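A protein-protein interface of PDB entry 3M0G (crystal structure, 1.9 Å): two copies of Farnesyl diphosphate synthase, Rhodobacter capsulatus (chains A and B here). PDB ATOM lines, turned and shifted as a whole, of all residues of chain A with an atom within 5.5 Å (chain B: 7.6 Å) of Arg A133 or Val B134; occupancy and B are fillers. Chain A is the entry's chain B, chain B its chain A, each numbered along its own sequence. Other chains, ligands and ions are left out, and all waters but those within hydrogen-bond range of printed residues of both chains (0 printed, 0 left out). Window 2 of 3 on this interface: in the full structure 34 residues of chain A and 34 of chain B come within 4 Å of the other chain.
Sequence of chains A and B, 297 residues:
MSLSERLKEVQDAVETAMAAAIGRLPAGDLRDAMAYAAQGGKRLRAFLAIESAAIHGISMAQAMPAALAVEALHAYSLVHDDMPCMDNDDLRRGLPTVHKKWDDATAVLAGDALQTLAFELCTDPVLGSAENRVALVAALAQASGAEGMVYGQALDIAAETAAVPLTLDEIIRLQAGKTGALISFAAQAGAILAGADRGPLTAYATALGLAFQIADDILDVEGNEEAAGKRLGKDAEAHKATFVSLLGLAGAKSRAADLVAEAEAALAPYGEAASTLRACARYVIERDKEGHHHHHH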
ATOM      1  N   CYS A 122     -12.132   6.839 -19.984  1.00  0.00           N
ATOM      2  CA  CYS A 122     -12.128   6.403 -18.570  1.00  0.00           C
ATOM      3  C   CYS A 122     -12.828   7.354 -17.592  1.00  0.00           C
ATOM      4  O   CYS A 122     -13.066   6.991 -16.433  1.00  0.00           O
ATOM      5  CB  CYS A 122     -10.688   6.161 -18.107  1.00  0.00           C
ATOM      6  SG  CYS A 122      -9.937   4.654 -18.855  1.00  0.00           S
ATOM      7  N   THR A 123     -13.142   8.561 -18.050  1.00  0.00           N
ATOM      8  CA  THR A 123     -13.693   9.603 -17.185  1.00  0.00           C
ATOM      9  C   THR A 123     -15.199   9.719 -17.313  1.00  0.00           C
ATOM     10  O   THR A 123     -15.830  10.414 -16.527  1.00  0.00           O
ATOM     11  CB  THR A 123     -13.115  11.001 -17.482  1.00  0.00           C
ATOM     12  OG1 THR A 123     -13.521  11.424 -18.786  1.00  0.00           O
ATOM     13  CG2 THR A 123     -11.579  11.039 -17.368  1.00  0.00           C
ATOM     14  N   ASP A 124     -15.757   9.064 -18.328  1.00  0.00           N
ATOM     15  CA  ASP A 124     -17.200   9.042 -18.586  1.00  0.00           C
ATOM     16  C   ASP A 124     -17.977   8.570 -17.363  1.00  0.00           C
ATOM     17  O   ASP A 124     -17.794   7.424 -16.925  1.00  0.00           O
ATOM     18  CB  ASP A 124     -17.486   8.104 -19.772  1.00  0.00           C
ATOM     19  CG  ASP A 124     -18.886   8.276 -20.345  1.00  0.00           C
ATOM     20  OD1 ASP A 124     -19.840   8.412 -19.569  1.00  0.00           O
ATOM     21  OD2 ASP A 124     -19.038   8.265 -21.585  1.00  0.00           O
ATOM     22  N   PRO A 125     -18.870   9.439 -16.827  1.00  0.00           N
ATOM     23  CA  PRO A 125     -19.613   9.125 -15.604  1.00  0.00           C
ATOM     24  C   PRO A 125     -20.552   7.934 -15.752  1.00  0.00           C
ATOM     25  O   PRO A 125     -20.929   7.342 -14.745  1.00  0.00           O
ATOM     26  CB  PRO A 125     -20.419  10.402 -15.334  1.00  0.00           C
ATOM     27  CG  PRO A 125     -20.446  11.128 -16.632  1.00  0.00           C
ATOM     28  CD  PRO A 125     -19.161  10.807 -17.299  1.00  0.00           C
ATOM     29  N   LEU A 127     -19.624   5.196 -16.510  1.00  0.00           N
ATOM     30  CA  LEU A 127     -18.832   4.138 -15.887  1.00  0.00           C
ATOM     31  C   LEU A 127     -19.118   3.928 -14.410  1.00  0.00           C
ATOM     32  O   LEU A 127     -18.879   2.839 -13.894  1.00  0.00           O
ATOM     33  CB  LEU A 127     -17.327   4.434 -16.044  1.00  0.00           C
ATOM     34  CG  LEU A 127     -16.711   4.244 -17.420  1.00  0.00           C
ATOM     35  CD1 LEU A 127     -15.377   4.970 -17.482  1.00  0.00           C
ATOM     36  CD2 LEU A 127     -16.542   2.762 -17.743  1.00  0.00           C
ATOM     37  N   GLY A 128     -19.595   4.970 -13.723  1.00  0.00           N
ATOM     38  CA  GLY A 128     -19.857   4.894 -12.285  1.00  0.00           C
ATOM     39  C   GLY A 128     -19.130   5.904 -11.413  1.00  0.00           C
ATOM     40  O   GLY A 128     -18.758   6.994 -11.874  1.00  0.00           O
ATOM     41  N   SER A 129     -18.914   5.546 -10.146  1.00  0.00           N
ATOM     42  CA  SER A 129     -18.347   6.481  -9.165  1.00  0.00           C
ATOM     43  C   SER A 129     -17.026   7.061  -9.652  1.00  0.00           C
ATOM     44  O   SER A 129     -16.315   6.411 -10.422  1.00  0.00           O
ATOM     45  CB  SER A 129     -18.181   5.813  -7.789  1.00  0.00           C
ATOM     46  OG  SER A 129     -17.055   4.951  -7.742  1.00  0.00           O
ATOM     47  N   ALA A 130     -16.721   8.291  -9.238  1.00  0.00           N
ATOM     48  CA  ALA A 130     -15.404   8.896  -9.507  1.00  0.00           C
ATOM     49  C   ALA A 130     -14.248   8.036  -8.978  1.00  0.00           C
ATOM     50  O   ALA A 130     -13.144   8.004  -9.578  1.00  0.00           O
ATOM     51  CB  ALA A 130     -15.332  10.303  -8.903  1.00  0.00           C
ATOM     52  N   GLU A 131     -14.495   7.391  -7.834  1.00  0.00           N
ATOM     53  CA  GLU A 131     -13.522   6.518  -7.177  1.00  0.00           C
ATOM     54  C   GLU A 131     -13.124   5.325  -8.054  1.00  0.00           C
ATOM     55  O   GLU A 131     -11.937   5.022  -8.203  1.00  0.00           O
ATOM     56  CB  GLU A 131     -14.087   6.006  -5.857  1.00  0.00           C
ATOM     57  CG  GLU A 131     -13.075   5.979  -4.720  1.00  0.00           C
ATOM     58  CD  GLU A 131     -12.937   7.324  -4.016  1.00  0.00           C
ATOM     59  OE1 GLU A 131     -13.883   8.145  -4.084  1.00  0.00           O
ATOM     60  OE2 GLU A 131     -11.886   7.552  -3.374  1.00  0.00           O
ATOM     61  N   ASN A 132     -14.120   4.640  -8.614  1.00  0.00           N
ATOM     62  CA  ASN A 132     -13.866   3.527  -9.547  1.00  0.00           C
ATOM     63  C   ASN A 132     -13.215   4.057 -10.835  1.00  0.00           C
ATOM     64  O   ASN A 132     -12.332   3.406 -11.407  1.00  0.00           O
ATOM     65  CB  ASN A 132     -15.171   2.749  -9.835  1.00  0.00           C
ATOM     66  CG  ASN A 132     -15.692   1.992  -8.612  1.00  0.00           C
ATOM     67  OD1 ASN A 132     -14.997   1.871  -7.604  1.00  0.00           O
ATOM     68  ND2 ASN A 132     -16.926   1.479  -8.701  1.00  0.00           N
ATOM     69  N   ARG A 133     -13.639   5.238 -11.290  1.00  0.00           N
ATOM     70  CA  ARG A 133     -13.085   5.805 -12.521  1.00  0.00           C
ATOM     71  C   ARG A 133     -11.606   6.144 -12.396  1.00  0.00           C
ATOM     72  O   ARG A 133     -10.836   5.874 -13.312  1.00  0.00           O
ATOM     73  CB  ARG A 133     -13.906   7.002 -13.021  1.00  0.00           C
ATOM     74  CG  ARG A 133     -15.236   6.608 -13.689  1.00  0.00           C
ATOM     75  CD  ARG A 133     -15.972   7.824 -14.225  1.00  0.00           C
ATOM     76  NE  ARG A 133     -16.779   8.460 -13.185  1.00  0.00           N
ATOM     77  CZ  ARG A 133     -17.066   9.758 -13.118  1.00  0.00           C
ATOM     78  NH1 ARG A 133     -16.598  10.610 -14.015  1.00  0.00           N
ATOM     79  NH2 ARG A 133     -17.820  10.207 -12.126  1.00  0.00           N
ATOM     80  N   VAL A 134     -11.203   6.696 -11.255  1.00  0.00           N
ATOM     81  CA  VAL A 134      -9.788   6.984 -11.059  1.00  0.00           C
ATOM     82  C   VAL A 134      -8.985   5.685 -10.925  1.00  0.00           C
ATOM     83  O   VAL A 134      -7.869   5.629 -11.365  1.00  0.00           O
ATOM     84  CB  VAL A 134      -9.531   7.959  -9.880  1.00  0.00           C
ATOM     85  CG1 VAL A 134      -9.648   7.256  -8.511  1.00  0.00           C
ATOM     86  CG2 VAL A 134      -8.157   8.606 -10.019  1.00  0.00           C
ATOM     87  N   ALA A 135      -9.559   4.655 -10.307  1.00  0.00           N
ATOM     88  CA  ALA A 135      -8.886   3.352 -10.221  1.00  0.00           C
ATOM     89  C   ALA A 135      -8.756   2.775 -11.629  1.00  0.00           C
ATOM     90  O   ALA A 135      -7.800   2.058 -11.920  1.00  0.00           O
ATOM     91  CB  ALA A 135      -9.658   2.406  -9.308  1.00  0.00           C
ATOM     92  N   LEU A 136      -9.739   3.068 -12.488  1.00  0.00           N
ATOM     93  CA  LEU A 136      -9.692   2.655 -13.894  1.00  0.00           C
ATOM     94  C   LEU A 136      -8.523   3.325 -14.656  1.00  0.00           C
ATOM     95  O   LEU A 136      -7.760   2.636 -15.340  1.00  0.00           O
ATOM     96  CB  LEU A 136     -11.048   2.884 -14.591  1.00  0.00           C
ATOM     97  CG  LEU A 136     -11.201   2.146 -15.925  1.00  0.00           C
ATOM     98  CD1 LEU A 136     -11.381   0.658 -15.666  1.00  0.00           C
ATOM     99  CD2 LEU A 136     -12.367   2.719 -16.728  1.00  0.00           C
ATOM    100  N   VAL A 137      -8.374   4.647 -14.503  1.00  0.00           N
ATOM    101  CA  VAL A 137      -7.268   5.429 -15.093  1.00  0.00           C
ATOM    102  C   VAL A 137      -5.906   4.942 -14.597  1.00  0.00           C
ATOM    103  O   VAL A 137      -4.986   4.763 -15.403  1.00  0.00           O
ATOM    104  CB  VAL A 137      -7.415   6.982 -14.817  1.00  0.00           C
ATOM    105  CG1 VAL A 137      -6.175   7.782 -15.269  1.00  0.00           C
ATOM    106  CG2 VAL A 137      -8.679   7.526 -15.473  1.00  0.00           C
ATOM    107  N   ALA A 138      -5.772   4.748 -13.277  1.00  0.00           N
ATOM    108  CA  ALA A 138      -4.511   4.274 -12.698  1.00  0.00           C
ATOM    109  C   ALA A 138      -4.136   2.911 -13.286  1.00  0.00           C
ATOM    110  O   ALA A 138      -2.990   2.678 -13.628  1.00  0.00           O
ATOM    111  CB  ALA A 138      -4.583   4.206 -11.157  1.00  0.00           C
ATOM    112  N   CYS B 122      -1.966  12.131 -12.508  1.00  0.00           N
ATOM    113  CA  CYS B 122      -3.316  12.654 -12.210  1.00  0.00           C
ATOM    114  C   CYS B 122      -4.189  11.798 -11.264  1.00  0.00           C
ATOM    115  O   CYS B 122      -5.192  12.291 -10.735  1.00  0.00           O
ATOM    116  CB  CYS B 122      -4.068  12.934 -13.522  1.00  0.00           C
ATOM    117  SG  CYS B 122      -3.340  14.244 -14.504  1.00  0.00           S
ATOM    118  N   THR B 123      -3.807  10.537 -11.050  1.00  0.00           N
ATOM    119  CA  THR B 123      -4.497   9.660 -10.096  1.00  0.00           C
ATOM    120  C   THR B 123      -3.922   9.671  -8.656  1.00  0.00           C
ATOM    121  O   THR B 123      -4.482   9.031  -7.768  1.00  0.00           O
ATOM    122  CB  THR B 123      -4.501   8.173 -10.566  1.00  0.00           C
ATOM    123  OG1 THR B 123      -3.185   7.624 -10.420  1.00  0.00           O
ATOM    124  CG2 THR B 123      -4.940   8.027 -12.008  1.00  0.00           C
ATOM    125  N   SER B 129      -9.621  14.577  -3.527  1.00  0.00           N
ATOM    126  CA  SER B 129     -10.744  13.679  -3.747  1.00  0.00           C
ATOM    127  C   SER B 129     -10.702  13.058  -5.133  1.00  0.00           C
ATOM    128  O   SER B 129     -10.142  13.629  -6.060  1.00  0.00           O
ATOM    129  CB  SER B 129     -12.074  14.422  -3.567  1.00  0.00           C
ATOM    130  OG  SER B 129     -12.284  15.350  -4.616  1.00  0.00           O
ATOM    131  N   ALA B 130     -11.327  11.893  -5.257  1.00  0.00           N
ATOM    132  CA  ALA B 130     -11.457  11.207  -6.530  1.00  0.00           C
ATOM    133  C   ALA B 130     -12.205  12.056  -7.566  1.00  0.00           C
ATOM    134  O   ALA B 130     -11.808  12.087  -8.735  1.00  0.00           O
ATOM    135  CB  ALA B 130     -12.131   9.852  -6.327  1.00  0.00           C
ATOM    136  N   GLU B 131     -13.260  12.764  -7.138  1.00  0.00           N
ATOM    137  CA  GLU B 131     -14.021  13.615  -8.055  1.00  0.00           C
ATOM    138  C   GLU B 131     -13.132  14.681  -8.678  1.00  0.00           C
ATOM    139  O   GLU B 131     -13.209  14.932  -9.879  1.00  0.00           O
ATOM    140  CB  GLU B 131     -15.253  14.253  -7.395  1.00  0.00           C
ATOM    141  CG  GLU B 131     -16.578  13.637  -7.851  1.00  0.00           C
ATOM    142  CD  GLU B 131     -17.153  12.601  -6.886  1.00  0.00           C
ATOM    143  OE1 GLU B 131     -18.391  12.421  -6.885  1.00  0.00           O
ATOM    144  OE2 GLU B 131     -16.387  11.980  -6.114  1.00  0.00           O
ATOM    145  N   ASN B 132     -12.268  15.277  -7.864  1.00  0.00           N
ATOM    146  CA  ASN B 132     -11.315  16.267  -8.373  1.00  0.00           C
ATOM    147  C   ASN B 132     -10.189  15.677  -9.256  1.00  0.00           C
ATOM    148  O   ASN B 132      -9.744  16.327 -10.214  1.00  0.00           O
ATOM    149  CB  ASN B 132     -10.809  17.164  -7.235  1.00  0.00           C
ATOM    150  CG  ASN B 132     -11.907  18.094  -6.692  1.00  0.00           C
ATOM    151  OD1 ASN B 132     -13.079  18.007  -7.101  1.00  0.00           O
ATOM    152  ND2 ASN B 132     -11.545  18.967  -5.761  1.00  0.00           N
ATOM    153  N   ARG B 133      -9.757  14.448  -8.956  1.00  0.00           N
ATOM    154  CA  ARG B 133      -8.760  13.777  -9.780  1.00  0.00           C
ATOM    155  C   ARG B 133      -9.316  13.405 -11.162  1.00  0.00           C
ATOM    156  O   ARG B 133      -8.636  13.602 -12.155  1.00  0.00           O
ATOM    157  CB  ARG B 133      -8.151  12.561  -9.065  1.00  0.00           C
ATOM    158  CG  ARG B 133      -7.157  12.935  -7.953  1.00  0.00           C
ATOM    159  CD  ARG B 133      -6.643  11.668  -7.219  1.00  0.00           C
ATOM    160  NE  ARG B 133      -7.597  11.184  -6.225  1.00  0.00           N
ATOM    161  CZ  ARG B 133      -7.576   9.981  -5.652  1.00  0.00           C
ATOM    162  NH1 ARG B 133      -6.674   9.073  -6.005  1.00  0.00           N
ATOM    163  NH2 ARG B 133      -8.497   9.672  -4.737  1.00  0.00           N
ATOM    164  N   VAL B 134     -10.557  12.903 -11.217  1.00  0.00           N
ATOM    165  CA  VAL B 134     -11.204  12.559 -12.488  1.00  0.00           C
ATOM    166  C   VAL B 134     -11.479  13.799 -13.360  1.00  0.00           C
ATOM    167  O   VAL B 134     -11.387  13.728 -14.587  1.00  0.00           O
ATOM    168  CB  VAL B 134     -12.486  11.693 -12.282  1.00  0.00           C
ATOM    169  CG1 VAL B 134     -13.638  12.520 -11.779  1.00  0.00           C
ATOM    170  CG2 VAL B 134     -12.875  10.959 -13.577  1.00  0.00           C
ATOM    171  N   ALA B 135     -11.808  14.910 -12.700  1.00  0.00           N
ATOM    172  CA  ALA B 135     -11.939  16.220 -13.328  1.00  0.00           C
ATOM    173  C   ALA B 135     -10.581  16.664 -13.862  1.00  0.00           C
ATOM    174  O   ALA B 135     -10.521  17.159 -14.974  1.00  0.00           O
ATOM    175  CB  ALA B 135     -12.471  17.244 -12.322  1.00  0.00           C
ATOM    176  N   LEU B 136      -9.514  16.440 -13.092  1.00  0.00           N
ATOM    177  CA  LEU B 136      -8.130  16.733 -13.551  1.00  0.00           C
ATOM    178  C   LEU B 136      -7.764  15.923 -14.817  1.00  0.00           C
ATOM    179  O   LEU B 136      -7.146  16.441 -15.764  1.00  0.00           O
ATOM    180  CB  LEU B 136      -7.112  16.441 -12.447  1.00  0.00           C
ATOM    181  CG  LEU B 136      -5.681  16.929 -12.752  1.00  0.00           C
ATOM    182  CD1 LEU B 136      -5.680  18.423 -12.791  1.00  0.00           C
ATOM    183  CD2 LEU B 136      -4.644  16.404 -11.736  1.00  0.00           C
ATOM    184  N   VAL B 137      -8.133  14.652 -14.802  1.00  0.00           N
ATOM    185  CA  VAL B 137      -7.916  13.733 -15.932  1.00  0.00           C
ATOM    186  C   VAL B 137      -8.639  14.199 -17.186  1.00  0.00           C
ATOM    187  O   VAL B 137      -8.007  14.317 -18.231  1.00  0.00           O
ATOM    188  CB  VAL B 137      -8.291  12.278 -15.564  1.00  0.00           C
ATOM    189  CG1 VAL B 137      -8.253  11.355 -16.801  1.00  0.00           C
ATOM    190  CG2 VAL B 137      -7.321  11.754 -14.507  1.00  0.00           C
ATOM    191  N   ALA B 138      -9.948  14.460 -17.091  1.00  0.00           N
ATOM    192  CA  ALA B 138     -10.719  14.930 -18.253  1.00  0.00           C
ATOM    193  C   ALA B 138     -10.139  16.196 -18.843  1.00  0.00           C
ATOM    194  O   ALA B 138      -9.993  16.278 -20.056  1.00  0.00           O
ATOM    195  CB  ALA B 138     -12.175  15.130 -17.931  1.00  0.00           C
ATOM    196  N   ALA B 139      -9.819  17.168 -17.977  1.00  0.00           N
ATOM    197  CA  ALA B 139      -9.239  18.435 -18.390  1.00  0.00           C
ATOM    198  C   ALA B 139      -7.884  18.240 -19.079  1.00  0.00           C
ATOM    199  O   ALA B 139      -7.579  18.927 -20.061  1.00  0.00           O
ATOM    200  CB  ALA B 139      -9.087  19.385 -17.169  1.00  0.00           C
ATOM    201  N   LEU B 140      -7.074  17.307 -18.567  1.00  0.00           N
ATOM    202  CA  LEU B 140      -5.802  16.999 -19.219  1.00  0.00           C
ATOM    203  C   LEU B 140      -6.015  16.409 -20.623  1.00  0.00           C
ATOM    204  O   LEU B 140      -5.386  16.848 -21.554  1.00  0.00           O
ATOM    205  CB  LEU B 140      -4.914  16.086 -18.352  1.00  0.00           C
ATOM    206  CG  LEU B 140      -3.533  15.766 -18.936  1.00  0.00           C
ATOM    207  CD1 LEU B 140      -2.775  17.040 -19.263  1.00  0.00           C
ATOM    208  CD2 LEU B 140      -2.716  14.877 -18.005  1.00  0.00           C
ATOM    209  N   ILE B 192      -9.320  23.413 -10.383  1.00  0.00           N
ATOM    210  CA  ILE B 192      -9.827  22.049 -10.498  1.00  0.00           C
ATOM    211  C   ILE B 192      -9.641  21.344  -9.173  1.00  0.00           C
ATOM    212  O   ILE B 192     -10.570  20.731  -8.671  1.00  0.00           O
ATOM    213  CB  ILE B 192      -9.166  21.267 -11.657  1.00  0.00           C
ATOM    214  CG1 ILE B 192      -9.588  21.884 -13.001  1.00  0.00           C
ATOM    215  CG2 ILE B 192      -9.532  19.737 -11.580  1.00  0.00           C
ATOM    216  CD1 ILE B 192      -8.788  21.425 -14.221  1.00  0.00           C
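Hydrophobic or aromatic side chains of chain A that line the printed part of chain B: Ala A130, Val A134, Val A137 and Ala A138. Printed residues of chain B that touch a printed residue of chain A: Thr B123, Ala B130, Glu B131, Val B134, Val B137 and Ala B138. Among the printed residues, 10 pairs touch across the chains. Among the printed residues, no Asp or Glu carboxylate lies within 4 Å of a Lys or Arg side-chain nitrogen of the other chain.
Thr A123 touches Val B134, and with the chains exchanged Val A134 touches Thr B123. Thr A123 touches Val B137, and with the chains exchanged Val A137 touches Thr B123. Thr A123 touches Ala B138, and with the chains exchanged Ala A138 touches Thr B123. Ala A130 touches Glu B131, and with the chains exchanged Glu A131 touches Ala B130. 12 positions are printed for both chains. Of the 10 pairs that touch across the chains among the printed residues, 9 have their exchanged pair printed and touching as well.
Of the printed residues of chain B, Thr A123 touches Val B134, Val B137 and Ala B138. Printed residues of chain B within 4 Å of Glu A131: Ala B130. Of chain B, only Val B134 (3.8 Å) comes within 4 Å of Arg A133. Printed residues of chain B within 4 Å of Val A137: Thr B123. Cys B122 touches none of the printed residues of chain A. Printed residues of chain A within 4 Å of Thr B123: Val A134 (3.7 Å), Val A137 (3.5 Å) and Ala A138 (3.6 Å). Printed residues of chain A within 4 Å of Val B134: Thr A123 and Arg A133. Leu B140 touches none of the printed residues of chain A.
The guanidinium group of Arg B133 sits at hydrogen-bond distance from the backbone carbonyl oxygen of Thr B123 (2.8 Å). The backbone carbonyl oxygen of Thr A123 lies within hydrogen-bond range of the guanidinium group of Arg A133, at 2.6 Å. The backbone carbonyl oxygen (O) of Gly A128 lies within hydrogen-bond range of the guanidinium group (NE) of Arg A133 (2.8 Å). The backbone carbonyl oxygen (O) of Ser A129 lies close to the guanidinium group (NE) of Arg A133, 3.5 Å away.
Val B134 touches Thr A123 (O to CG2, 3.9 Å). Thr A123 touches Val B137 (CG2 to CG1, 3.4 Å). Thr A123 touches Ala B138 (CG2 to N, 3.8 Å). Ala A130 touches Ala B130. Glu B131 touches Ala A130. Ala B130 touches Glu A131 (CB to OE1, 3.3 Å). Val B134 touches Arg A133 (CG2 to NH1, 3.8 Å). Val A134 touches Thr B123 (CG2 to CB, 3.7 Å). Val A137 touches Thr B123. N of Ala A138 touches CG2 of Thr B123 (3.6 Å).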
